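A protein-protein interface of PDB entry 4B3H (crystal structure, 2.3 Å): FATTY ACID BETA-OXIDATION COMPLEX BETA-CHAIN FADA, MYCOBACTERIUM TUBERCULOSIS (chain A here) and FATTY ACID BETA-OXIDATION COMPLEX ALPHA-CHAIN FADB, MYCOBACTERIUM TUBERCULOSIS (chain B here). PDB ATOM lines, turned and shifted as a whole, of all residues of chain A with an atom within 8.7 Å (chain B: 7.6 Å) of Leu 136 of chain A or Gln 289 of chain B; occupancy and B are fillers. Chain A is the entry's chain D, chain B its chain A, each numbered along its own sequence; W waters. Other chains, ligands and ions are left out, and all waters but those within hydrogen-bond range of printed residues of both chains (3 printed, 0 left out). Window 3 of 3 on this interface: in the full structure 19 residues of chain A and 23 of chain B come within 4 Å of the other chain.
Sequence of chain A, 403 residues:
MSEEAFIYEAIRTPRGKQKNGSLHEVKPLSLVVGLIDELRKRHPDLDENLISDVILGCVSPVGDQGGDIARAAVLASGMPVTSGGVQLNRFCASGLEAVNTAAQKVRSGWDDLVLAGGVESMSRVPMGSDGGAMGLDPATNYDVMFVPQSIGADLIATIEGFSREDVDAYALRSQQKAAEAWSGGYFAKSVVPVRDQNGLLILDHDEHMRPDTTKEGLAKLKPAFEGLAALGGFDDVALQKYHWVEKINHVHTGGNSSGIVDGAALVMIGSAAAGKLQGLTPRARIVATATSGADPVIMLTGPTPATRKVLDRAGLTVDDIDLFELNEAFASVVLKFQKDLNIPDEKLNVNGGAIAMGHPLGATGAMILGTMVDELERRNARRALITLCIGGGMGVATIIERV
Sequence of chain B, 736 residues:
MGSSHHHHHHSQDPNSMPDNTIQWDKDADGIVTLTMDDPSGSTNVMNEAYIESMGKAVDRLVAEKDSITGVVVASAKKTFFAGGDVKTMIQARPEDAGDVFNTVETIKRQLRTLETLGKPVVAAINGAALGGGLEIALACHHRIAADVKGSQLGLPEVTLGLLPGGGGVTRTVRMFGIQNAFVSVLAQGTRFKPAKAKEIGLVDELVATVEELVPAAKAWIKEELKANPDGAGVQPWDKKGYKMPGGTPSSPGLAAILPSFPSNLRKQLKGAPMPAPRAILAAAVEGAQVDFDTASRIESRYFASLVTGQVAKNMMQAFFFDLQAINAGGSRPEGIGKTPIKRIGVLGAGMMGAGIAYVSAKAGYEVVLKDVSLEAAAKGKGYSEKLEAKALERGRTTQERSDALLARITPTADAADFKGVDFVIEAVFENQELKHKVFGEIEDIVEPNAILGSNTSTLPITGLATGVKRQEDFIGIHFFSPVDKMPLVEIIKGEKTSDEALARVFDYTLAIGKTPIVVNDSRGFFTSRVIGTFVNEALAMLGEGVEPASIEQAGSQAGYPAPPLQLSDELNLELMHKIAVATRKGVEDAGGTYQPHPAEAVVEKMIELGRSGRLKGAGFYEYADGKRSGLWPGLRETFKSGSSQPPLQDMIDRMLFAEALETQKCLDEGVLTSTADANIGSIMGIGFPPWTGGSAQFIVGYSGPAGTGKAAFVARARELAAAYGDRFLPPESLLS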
ATOM      1  N   GLY A 128     -34.676 -12.987   2.328  1.00  0.00           N
ATOM      2  CA  GLY A 128     -33.910 -11.782   2.007  1.00  0.00           C
ATOM      3  C   GLY A 128     -34.637 -10.474   2.275  1.00  0.00           C
ATOM      4  O   GLY A 128     -34.050  -9.406   2.136  1.00  0.00           O
ATOM      5  N   SER A 129     -35.909 -10.557   2.658  1.00  0.00           N
ATOM      6  CA  SER A 129     -36.718  -9.382   3.000  1.00  0.00           C
ATOM      7  C   SER A 129     -36.132  -8.524   4.113  1.00  0.00           C
ATOM      8  O   SER A 129     -36.444  -7.338   4.202  1.00  0.00           O
ATOM      9  CB  SER A 129     -38.119  -9.807   3.431  1.00  0.00           C
ATOM     10  OG  SER A 129     -38.913 -10.126   2.316  1.00  0.00           O
ATOM     11  N   ASP A 130     -35.312  -9.131   4.967  1.00  0.00           N
ATOM     12  CA  ASP A 130     -34.764  -8.446   6.136  1.00  0.00           C
ATOM     13  C   ASP A 130     -33.468  -7.684   5.851  1.00  0.00           C
ATOM     14  O   ASP A 130     -32.858  -7.120   6.761  1.00  0.00           O
ATOM     15  CB  ASP A 130     -34.583  -9.425   7.304  1.00  0.00           C
ATOM     16  CG  ASP A 130     -33.597 -10.536   6.999  1.00  0.00           C
ATOM     17  OD1 ASP A 130     -33.705 -11.161   5.922  1.00  0.00           O
ATOM     18  OD2 ASP A 130     -32.721 -10.794   7.852  1.00  0.00           O
ATOM     19  N   GLY A 131     -33.069  -7.653   4.582  1.00  0.00           N
ATOM     20  CA  GLY A 131     -31.835  -6.992   4.171  1.00  0.00           C
ATOM     21  C   GLY A 131     -30.661  -7.917   4.397  1.00  0.00           C
ATOM     22  O   GLY A 131     -30.540  -8.949   3.740  1.00  0.00           O
ATOM     23  N   GLY A 132     -29.794  -7.556   5.334  1.00  0.00           N
ATOM     24  CA  GLY A 132     -28.673  -8.410   5.673  1.00  0.00           C
ATOM     25  C   GLY A 132     -27.399  -7.621   5.827  1.00  0.00           C
ATOM     26  O   GLY A 132     -26.954  -6.951   4.896  1.00  0.00           O
ATOM     27  N   ALA A 133     -26.821  -7.714   7.020  1.00  0.00           N
ATOM     28  CA  ALA A 133     -25.592  -7.010   7.365  1.00  0.00           C
ATOM     29  C   ALA A 133     -24.474  -7.269   6.354  1.00  0.00           C
ATOM     30  O   ALA A 133     -23.745  -6.352   5.992  1.00  0.00           O
ATOM     31  CB  ALA A 133     -25.152  -7.394   8.773  1.00  0.00           C
ATOM     32  N   MET A 134     -24.360  -8.515   5.895  1.00  0.00           N
ATOM     33  CA  MET A 134     -23.342  -8.904   4.918  1.00  0.00           C
ATOM     34  C   MET A 134     -23.591  -8.255   3.554  1.00  0.00           C
ATOM     35  O   MET A 134     -22.696  -7.611   3.009  1.00  0.00           O
ATOM     36  CB  MET A 134     -23.237 -10.438   4.808  1.00  0.00           C
ATOM     37  CG  MET A 134     -22.569 -11.099   6.015  1.00  0.00           C
ATOM     38  SD  MET A 134     -22.574 -12.913   6.101  1.00  0.00           S
ATOM     39  CE  MET A 134     -24.047 -13.269   7.060  1.00  0.00           C
ATOM     40  N   GLY A 135     -24.809  -8.405   3.030  1.00  0.00           N
ATOM     41  CA  GLY A 135     -25.173  -7.919   1.689  1.00  0.00           C
ATOM     42  C   GLY A 135     -25.183  -6.410   1.496  1.00  0.00           C
ATOM     43  O   GLY A 135     -24.762  -5.914   0.452  1.00  0.00           O
ATOM     44  N   LEU A 136     -25.665  -5.676   2.498  1.00  0.00           N
ATOM     45  CA  LEU A 136     -25.678  -4.204   2.458  1.00  0.00           C
ATOM     46  C   LEU A 136     -24.290  -3.603   2.689  1.00  0.00           C
ATOM     47  O   LEU A 136     -24.136  -2.378   2.784  1.00  0.00           O
ATOM     48  CB  LEU A 136     -26.662  -3.638   3.489  1.00  0.00           C
ATOM     49  CG  LEU A 136     -28.137  -3.475   3.104  1.00  0.00           C
ATOM     50  CD1 LEU A 136     -28.896  -4.793   3.168  1.00  0.00           C
ATOM     51  CD2 LEU A 136     -28.781  -2.451   4.024  1.00  0.00           C
ATOM     52  N   ASP A 137     -23.288  -4.472   2.774  1.00  0.00           N
ATOM     53  CA  ASP A 137     -21.929  -4.059   3.068  1.00  0.00           C
ATOM     54  C   ASP A 137     -20.947  -4.684   2.068  1.00  0.00           C
ATOM     55  O   ASP A 137     -20.425  -5.777   2.312  1.00  0.00           O
ATOM     56  CB  ASP A 137     -21.576  -4.444   4.505  1.00  0.00           C
ATOM     57  CG  ASP A 137     -20.347  -3.732   5.019  1.00  0.00           C
ATOM     58  OD1 ASP A 137     -19.878  -2.791   4.353  1.00  0.00           O
ATOM     59  OD2 ASP A 137     -19.848  -4.110   6.098  1.00  0.00           O
ATOM     60  N   PRO A 138     -20.707  -4.000   0.929  1.00  0.00           N
ATOM     61  CA  PRO A 138     -19.748  -4.475  -0.069  1.00  0.00           C
ATOM     62  C   PRO A 138     -18.367  -4.809   0.498  1.00  0.00           C
ATOM     63  O   PRO A 138     -17.774  -5.803   0.089  1.00  0.00           O
ATOM     64  CB  PRO A 138     -19.662  -3.306  -1.048  1.00  0.00           C
ATOM     65  CG  PRO A 138     -21.019  -2.714  -0.999  1.00  0.00           C
ATOM     66  CD  PRO A 138     -21.457  -2.830   0.435  1.00  0.00           C
ATOM     67  N   ALA A 139     -17.874  -3.998   1.434  1.00  0.00           N
ATOM     68  CA  ALA A 139     -16.580  -4.243   2.083  1.00  0.00           C
ATOM     69  C   ALA A 139     -16.546  -5.571   2.849  1.00  0.00           C
ATOM     70  O   ALA A 139     -15.525  -6.257   2.860  1.00  0.00           O
ATOM     71  CB  ALA A 139     -16.208  -3.086   3.001  1.00  0.00           C
ATOM     72  N   THR A 140     -17.665  -5.921   3.482  1.00  0.00           N
ATOM     73  CA  THR A 140     -17.819  -7.207   4.161  1.00  0.00           C
ATOM     74  C   THR A 140     -18.010  -8.326   3.140  1.00  0.00           C
ATOM     75  O   THR A 140     -17.252  -9.298   3.132  1.00  0.00           O
ATOM     76  CB  THR A 140     -19.010  -7.178   5.150  1.00  0.00           C
ATOM     77  OG1 THR A 140     -18.674  -6.351   6.270  1.00  0.00           O
ATOM     78  CG2 THR A 140     -19.376  -8.586   5.648  1.00  0.00           C
ATOM     79  N   ASN A 141     -19.025  -8.165   2.288  1.00  0.00           N
ATOM     80  CA  ASN A 141     -19.363  -9.110   1.226  1.00  0.00           C
ATOM     81  C   ASN A 141     -18.148  -9.517   0.379  1.00  0.00           C
ATOM     82  O   ASN A 141     -17.984 -10.690   0.049  1.00  0.00           O
ATOM     83  CB  ASN A 141     -20.464  -8.505   0.345  1.00  0.00           C
ATOM     84  CG  ASN A 141     -21.154  -9.531  -0.537  1.00  0.00           C
ATOM     85  OD1 ASN A 141     -20.542 -10.130  -1.422  1.00  0.00           O
ATOM     86  ND2 ASN A 141     -22.452  -9.713  -0.318  1.00  0.00           N
ATOM     87  N   VAL B 173     -23.012   9.125  -7.763  1.00  0.00           N
ATOM     88  CA  VAL B 173     -24.002   8.198  -7.205  1.00  0.00           C
ATOM     89  C   VAL B 173     -25.341   8.908  -6.981  1.00  0.00           C
ATOM     90  O   VAL B 173     -26.403   8.359  -7.273  1.00  0.00           O
ATOM     91  CB  VAL B 173     -23.488   7.515  -5.911  1.00  0.00           C
ATOM     92  CG1 VAL B 173     -24.602   6.757  -5.201  1.00  0.00           C
ATOM     93  CG2 VAL B 173     -22.348   6.565  -6.239  1.00  0.00           C
ATOM     94  N   ARG B 174     -25.281  10.137  -6.485  1.00  0.00           N
ATOM     95  CA  ARG B 174     -26.474  10.945  -6.289  1.00  0.00           C
ATOM     96  C   ARG B 174     -27.149  11.286  -7.632  1.00  0.00           C
ATOM     97  O   ARG B 174     -28.375  11.393  -7.709  1.00  0.00           O
ATOM     98  CB  ARG B 174     -26.114  12.220  -5.524  1.00  0.00           C
ATOM     99  CG  ARG B 174     -26.894  12.415  -4.237  1.00  0.00           C
ATOM    100  CD  ARG B 174     -26.538  11.367  -3.200  1.00  0.00           C
ATOM    101  NE  ARG B 174     -27.211  11.584  -1.923  1.00  0.00           N
ATOM    102  CZ  ARG B 174     -26.937  10.914  -0.806  1.00  0.00           C
ATOM    103  NH1 ARG B 174     -26.000   9.970  -0.799  1.00  0.00           N
ATOM    104  NH2 ARG B 174     -27.603  11.190   0.309  1.00  0.00           N
ATOM    105  N   ILE B 178     -26.221   4.003  -7.739  1.00  0.00           N
ATOM    106  CA  ILE B 178     -25.057   3.165  -7.445  1.00  0.00           C
ATOM    107  C   ILE B 178     -24.511   2.434  -8.674  1.00  0.00           C
ATOM    108  O   ILE B 178     -23.356   2.631  -9.056  1.00  0.00           O
ATOM    109  CB  ILE B 178     -25.356   2.163  -6.301  1.00  0.00           C
ATOM    110  CG1 ILE B 178     -25.616   2.921  -4.993  1.00  0.00           C
ATOM    111  CG2 ILE B 178     -24.203   1.177  -6.127  1.00  0.00           C
ATOM    112  CD1 ILE B 178     -26.403   2.137  -3.969  1.00  0.00           C
ATOM    113  N   MET B 244     -33.186   8.672  -5.419  1.00  0.00           N
ATOM    114  CA  MET B 244     -31.992   8.156  -6.067  1.00  0.00           C
ATOM    115  C   MET B 244     -32.386   7.259  -7.240  1.00  0.00           C
ATOM    116  O   MET B 244     -33.194   6.343  -7.066  1.00  0.00           O
ATOM    117  CB  MET B 244     -31.128   7.382  -5.064  1.00  0.00           C
ATOM    118  CG  MET B 244     -29.814   6.863  -5.637  1.00  0.00           C
ATOM    119  SD  MET B 244     -28.654   6.297  -4.377  1.00  0.00           S
ATOM    120  CE  MET B 244     -28.262   7.837  -3.551  1.00  0.00           C
ATOM    121  N   THR B 248     -32.266   3.544  -3.343  1.00  0.00           N
ATOM    122  CA  THR B 248     -31.264   3.397  -2.293  1.00  0.00           C
ATOM    123  C   THR B 248     -31.147   1.904  -1.961  1.00  0.00           C
ATOM    124  O   THR B 248     -31.982   1.113  -2.410  1.00  0.00           O
ATOM    125  CB  THR B 248     -31.658   4.193  -1.031  1.00  0.00           C
ATOM    126  OG1 THR B 248     -32.950   3.769  -0.583  1.00  0.00           O
ATOM    127  CG2 THR B 248     -31.687   5.690  -1.316  1.00  0.00           C
ATOM    128  N   PRO B 249     -30.114   1.501  -1.189  1.00  0.00           N
ATOM    129  CA  PRO B 249     -29.975   0.077  -0.854  1.00  0.00           C
ATOM    130  C   PRO B 249     -31.181  -0.536  -0.129  1.00  0.00           C
ATOM    131  O   PRO B 249     -31.377  -1.750  -0.188  1.00  0.00           O
ATOM    132  CB  PRO B 249     -28.739   0.050   0.051  1.00  0.00           C
ATOM    133  CG  PRO B 249     -27.939   1.225  -0.391  1.00  0.00           C
ATOM    134  CD  PRO B 249     -28.955   2.281  -0.717  1.00  0.00           C
ATOM    135  N   SER B 250     -31.979   0.292   0.541  1.00  0.00           N
ATOM    136  CA  SER B 250     -33.159  -0.191   1.262  1.00  0.00           C
ATOM    137  C   SER B 250     -34.391  -0.407   0.370  1.00  0.00           C
ATOM    138  O   SER B 250     -35.377  -1.008   0.805  1.00  0.00           O
ATOM    139  CB  SER B 250     -33.494   0.741   2.432  1.00  0.00           C
ATOM    140  OG  SER B 250     -33.829   2.038   1.976  1.00  0.00           O
ATOM    141  N   ALA B 255     -32.103  -3.747  -3.595  1.00  0.00           N
ATOM    142  CA  ALA B 255     -31.751  -4.704  -2.543  1.00  0.00           C
ATOM    143  C   ALA B 255     -31.625  -6.137  -3.069  1.00  0.00           C
ATOM    144  O   ALA B 255     -30.810  -6.917  -2.569  1.00  0.00           O
ATOM    145  CB  ALA B 255     -32.760  -4.636  -1.406  1.00  0.00           C
ATOM    146  N   LEU B 258     -28.165  -5.955  -5.266  1.00  0.00           N
ATOM    147  CA  LEU B 258     -27.009  -5.373  -4.574  1.00  0.00           C
ATOM    148  C   LEU B 258     -25.944  -6.372  -4.072  1.00  0.00           C
ATOM    149  O   LEU B 258     -24.752  -6.136  -4.275  1.00  0.00           O
ATOM    150  CB  LEU B 258     -27.475  -4.468  -3.427  1.00  0.00           C
ATOM    151  CG  LEU B 258     -26.421  -3.661  -2.669  1.00  0.00           C
ATOM    152  CD1 LEU B 258     -25.895  -2.525  -3.531  1.00  0.00           C
ATOM    153  CD2 LEU B 258     -27.004  -3.132  -1.368  1.00  0.00           C
ATOM    154  N   PRO B 259     -26.362  -7.479  -3.416  1.00  0.00           N
ATOM    155  CA  PRO B 259     -25.371  -8.443  -2.916  1.00  0.00           C
ATOM    156  C   PRO B 259     -24.505  -9.073  -4.009  1.00  0.00           C
ATOM    157  O   PRO B 259     -23.458  -9.653  -3.705  1.00  0.00           O
ATOM    158  CB  PRO B 259     -26.237  -9.521  -2.255  1.00  0.00           C
ATOM    159  CG  PRO B 259     -27.493  -8.817  -1.882  1.00  0.00           C
ATOM    160  CD  PRO B 259     -27.728  -7.856  -3.006  1.00  0.00           C
ATOM    161  N   ALA B 282     -17.745   0.204  -1.932  1.00  0.00           N
ATOM    162  CA  ALA B 282     -18.097   0.384  -0.521  1.00  0.00           C
ATOM    163  C   ALA B 282     -18.510   1.832  -0.235  1.00  0.00           C
ATOM    164  O   ALA B 282     -19.557   2.071   0.368  1.00  0.00           O
ATOM    165  CB  ALA B 282     -16.939  -0.039   0.375  1.00  0.00           C
ATOM    166  N   ALA B 283     -17.702   2.790  -0.694  1.00  0.00           N
ATOM    167  CA  ALA B 283     -18.005   4.218  -0.517  1.00  0.00           C
ATOM    168  C   ALA B 283     -19.325   4.605  -1.185  1.00  0.00           C
ATOM    169  O   ALA B 283     -20.100   5.387  -0.628  1.00  0.00           O
ATOM    170  CB  ALA B 283     -16.868   5.089  -1.044  1.00  0.00           C
ATOM    171  N   ALA B 284     -19.573   4.048  -2.370  1.00  0.00           N
ATOM    172  CA  ALA B 284     -20.804   4.309  -3.112  1.00  0.00           C
ATOM    173  C   ALA B 284     -22.043   3.821  -2.361  1.00  0.00           C
ATOM    174  O   ALA B 284     -22.978   4.591  -2.140  1.00  0.00           O
ATOM    175  CB  ALA B 284     -20.734   3.687  -4.501  1.00  0.00           C
ATOM    176  N   VAL B 285     -22.041   2.553  -1.963  1.00  0.00           N
ATOM    177  CA  VAL B 285     -23.193   1.951  -1.283  1.00  0.00           C
ATOM    178  C   VAL B 285     -23.423   2.570   0.098  1.00  0.00           C
ATOM    179  O   VAL B 285     -24.545   2.975   0.422  1.00  0.00           O
ATOM    180  CB  VAL B 285     -23.068   0.414  -1.197  1.00  0.00           C
ATOM    181  CG1 VAL B 285     -24.169  -0.178  -0.328  1.00  0.00           C
ATOM    182  CG2 VAL B 285     -23.107  -0.200  -2.590  1.00  0.00           C
ATOM    183  N   GLU B 286     -22.359   2.661   0.894  1.00  0.00           N
ATOM    184  CA  GLU B 286     -22.444   3.254   2.233  1.00  0.00           C
ATOM    185  C   GLU B 286     -22.899   4.707   2.145  1.00  0.00           C
ATOM    186  O   GLU B 286     -23.734   5.146   2.930  1.00  0.00           O
ATOM    187  CB  GLU B 286     -21.108   3.148   2.978  1.00  0.00           C
ATOM    188  CG  GLU B 286     -20.728   1.728   3.386  1.00  0.00           C
ATOM    189  CD  GLU B 286     -19.384   1.643   4.098  1.00  0.00           C
ATOM    190  OE1 GLU B 286     -19.000   2.603   4.803  1.00  0.00           O
ATOM    191  OE2 GLU B 286     -18.706   0.601   3.965  1.00  0.00           O
ATOM    192  N   GLY B 287     -22.361   5.442   1.174  1.00  0.00           N
ATOM    193  CA  GLY B 287     -22.795   6.814   0.922  1.00  0.00           C
ATOM    194  C   GLY B 287     -24.286   6.922   0.627  1.00  0.00           C
ATOM    195  O   GLY B 287     -24.961   7.824   1.125  1.00  0.00           O
ATOM    196  N   ALA B 288     -24.795   5.986  -0.172  1.00  0.00           N
ATOM    197  CA  ALA B 288     -26.211   5.947  -0.542  1.00  0.00           C
ATOM    198  C   ALA B 288     -27.160   5.685   0.631  1.00  0.00           C
ATOM    199  O   ALA B 288     -28.345   5.998   0.545  1.00  0.00           O
ATOM    200  CB  ALA B 288     -26.438   4.922  -1.637  1.00  0.00           C
ATOM    201  N   GLN B 289     -26.643   5.122   1.722  1.00  0.00           N
ATOM    202  CA  GLN B 289     -27.479   4.801   2.886  1.00  0.00           C
ATOM    203  C   GLN B 289     -27.762   6.001   3.799  1.00  0.00           C
ATOM    204  O   GLN B 289     -28.652   5.946   4.646  1.00  0.00           O
ATOM    205  CB  GLN B 289     -26.841   3.681   3.702  1.00  0.00           C
ATOM    206  CG  GLN B 289     -26.860   2.325   3.021  1.00  0.00           C
ATOM    207  CD  GLN B 289     -26.173   1.264   3.849  1.00  0.00           C
ATOM    208  OE1 GLN B 289     -24.950   1.255   3.971  1.00  0.00           O
ATOM    209  NE2 GLN B 289     -26.958   0.362   4.425  1.00  0.00           N
ATOM    210  N   VAL B 290     -27.005   7.080   3.623  1.00  0.00           N
ATOM    211  CA  VAL B 290     -27.054   8.219   4.537  1.00  0.00           C
ATOM    212  C   VAL B 290     -27.212   9.550   3.804  1.00  0.00           C
ATOM    213  O   VAL B 290     -27.141   9.600   2.575  1.00  0.00           O
ATOM    214  CB  VAL B 290     -25.788   8.278   5.426  1.00  0.00           C
ATOM    215  CG1 VAL B 290     -25.826   7.188   6.491  1.00  0.00           C
ATOM    216  CG2 VAL B 290     -24.518   8.185   4.580  1.00  0.00           C
ATOM    217  N   ASP B 291     -27.411  10.624   4.572  1.00  0.00           N
ATOM    218  CA  ASP B 291     -27.464  11.991   4.037  1.00  0.00           C
ATOM    219  C   ASP B 291     -26.156  12.372   3.329  1.00  0.00           C
ATOM    220  O   ASP B 291     -25.122  11.729   3.526  1.00  0.00           O
ATOM    221  CB  ASP B 291     -27.750  12.992   5.160  1.00  0.00           C
ATOM    222  CG  ASP B 291     -26.603  13.089   6.153  1.00  0.00           C
ATOM    223  OD1 ASP B 291     -26.503  12.211   7.037  1.00  0.00           O
ATOM    224  OD2 ASP B 291     -25.788  14.031   6.036  1.00  0.00           O
ATOM    225  N   THR B 294     -22.753  13.102   5.444  1.00  0.00           N
ATOM    226  CA  THR B 294     -22.222  11.860   6.013  1.00  0.00           C
ATOM    227  C   THR B 294     -21.617  10.988   4.911  1.00  0.00           C
ATOM    228  O   THR B 294     -20.536  10.426   5.081  1.00  0.00           O
ATOM    229  CB  THR B 294     -23.303  11.077   6.788  1.00  0.00           C
ATOM    230  OG1 THR B 294     -23.883  11.924   7.786  1.00  0.00           O
ATOM    231  CG2 THR B 294     -22.709   9.856   7.472  1.00  0.00           C
ATOM    232  N   ALA B 295     -22.317  10.894   3.781  1.00  0.00           N
ATOM    233  CA  ALA B 295     -21.836  10.152   2.615  1.00  0.00           C
ATOM    234  C   ALA B 295     -20.471  10.676   2.175  1.00  0.00           C
ATOM    235  O   ALA B 295     -19.566   9.902   1.856  1.00  0.00           O
ATOM    236  CB  ALA B 295     -22.836  10.267   1.476  1.00  0.00           C
ATOM    237  N   ILE B 298     -17.624   9.618   4.703  1.00  0.00           N
ATOM    238  CA  ILE B 298     -17.272   8.210   4.476  1.00  0.00           C
ATOM    239  C   ILE B 298     -16.322   8.093   3.280  1.00  0.00           C
ATOM    240  O   ILE B 298     -15.327   7.361   3.338  1.00  0.00           O
ATOM    241  CB  ILE B 298     -18.528   7.331   4.268  1.00  0.00           C
ATOM    242  CG1 ILE B 298     -19.339   7.247   5.573  1.00  0.00           C
ATOM    243  CG2 ILE B 298     -18.148   5.937   3.783  1.00  0.00           C
ATOM    244  CD1 ILE B 298     -20.770   6.785   5.404  1.00  0.00           C
HETATM  245  O   HOH W   1     -18.567  -1.346   6.272  1.00  0.00           O
HETATM  246  O   HOH W   2     -23.210  -5.376  -1.882  1.00  0.00           O
HETATM  247  O   HOH W   3     -19.078  -1.599   2.240  1.00  0.00           O
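The side-chain hydroxyl (OG1) of Thr 140 of chain A sits at hydrogen-bond distance from the side-chain carboxylate (OD2) of Asp 137 of chain A (2.5 Å).
Leu 136 of chain A touches Val 285 of chain B.
CD2 of Leu 136 of chain A touches NE2 of Gln 289 of chain B (3.4 Å).
Asp 137 of chain A touches Glu 286 of chain B.
Pro 138 of chain A touches Val 285 of chain B (CG to CG2, 3.6 Å).
ND2 of Asn 141 of chain A touches O of Pro 259 of chain B, 3.5 Å away.
Water W3 lies within hydrogen-bond range of the side-chain carboxylate (OD1) of Asp 137 of chain A (2.6 Å), the backbone NH (N) of Ala 139 of chain A (2.8 Å) and the side-chain carboxylate (OE2) of Glu 286 of chain B (2.8 Å).
Water W1 bridges OD1 of Asp 137 of chain A and OE2 of Glu 286 of chain B.
Water W2 bridges the backbone carbonyl oxygen of Gly 135 of chain A (2.9 Å) and the backbone carbonyl oxygen of Leu 258 of chain B (2.9 Å).
Leu 136 of chain A touches two residues of chain B.
Gly 287 of chain B touches none of the printed residues of chain A.
No residue of chain A comes within 4 Å of Ala 288 of chain B.
No residue of chain A comes within 4 Å of Val 290 of chain B.
Of the printed residues of chain A, Pro 259 of chain B touches Asn 141.
Of the printed residues of chain A, Val 285 of chain B touches Leu 136 and Pro 138.
Of the printed residues of chain B, Asp 137 of chain A touches Glu 286 (3.6 Å).
Of the printed residues of chain A, Glu 286 of chain B touches Asp 137 (3.6 Å).
Printed residues of chain B within 4 Å of Pro 138 of chain A: Val 285.
Val 173 of chain B touches none of the printed residues of chain A.
Gly 132 of chain A touches none of the printed residues of chain B.
The nearest printed residue of chain A that does not touch Glu 286 of chain B is Ala 139 of chain A (4.6 Å).
Of the 14 printed residues of chain A, 4 touch a printed residue of chain B.
Hydrophobic or aromatic side chains of chain A that line the printed part of chain B: Leu 136 and Pro 138.
Hydrophobic or aromatic side chains of chain B that line the printed part of chain A: Val 285.
Among the printed residues, 5 pairs touch across the chains.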
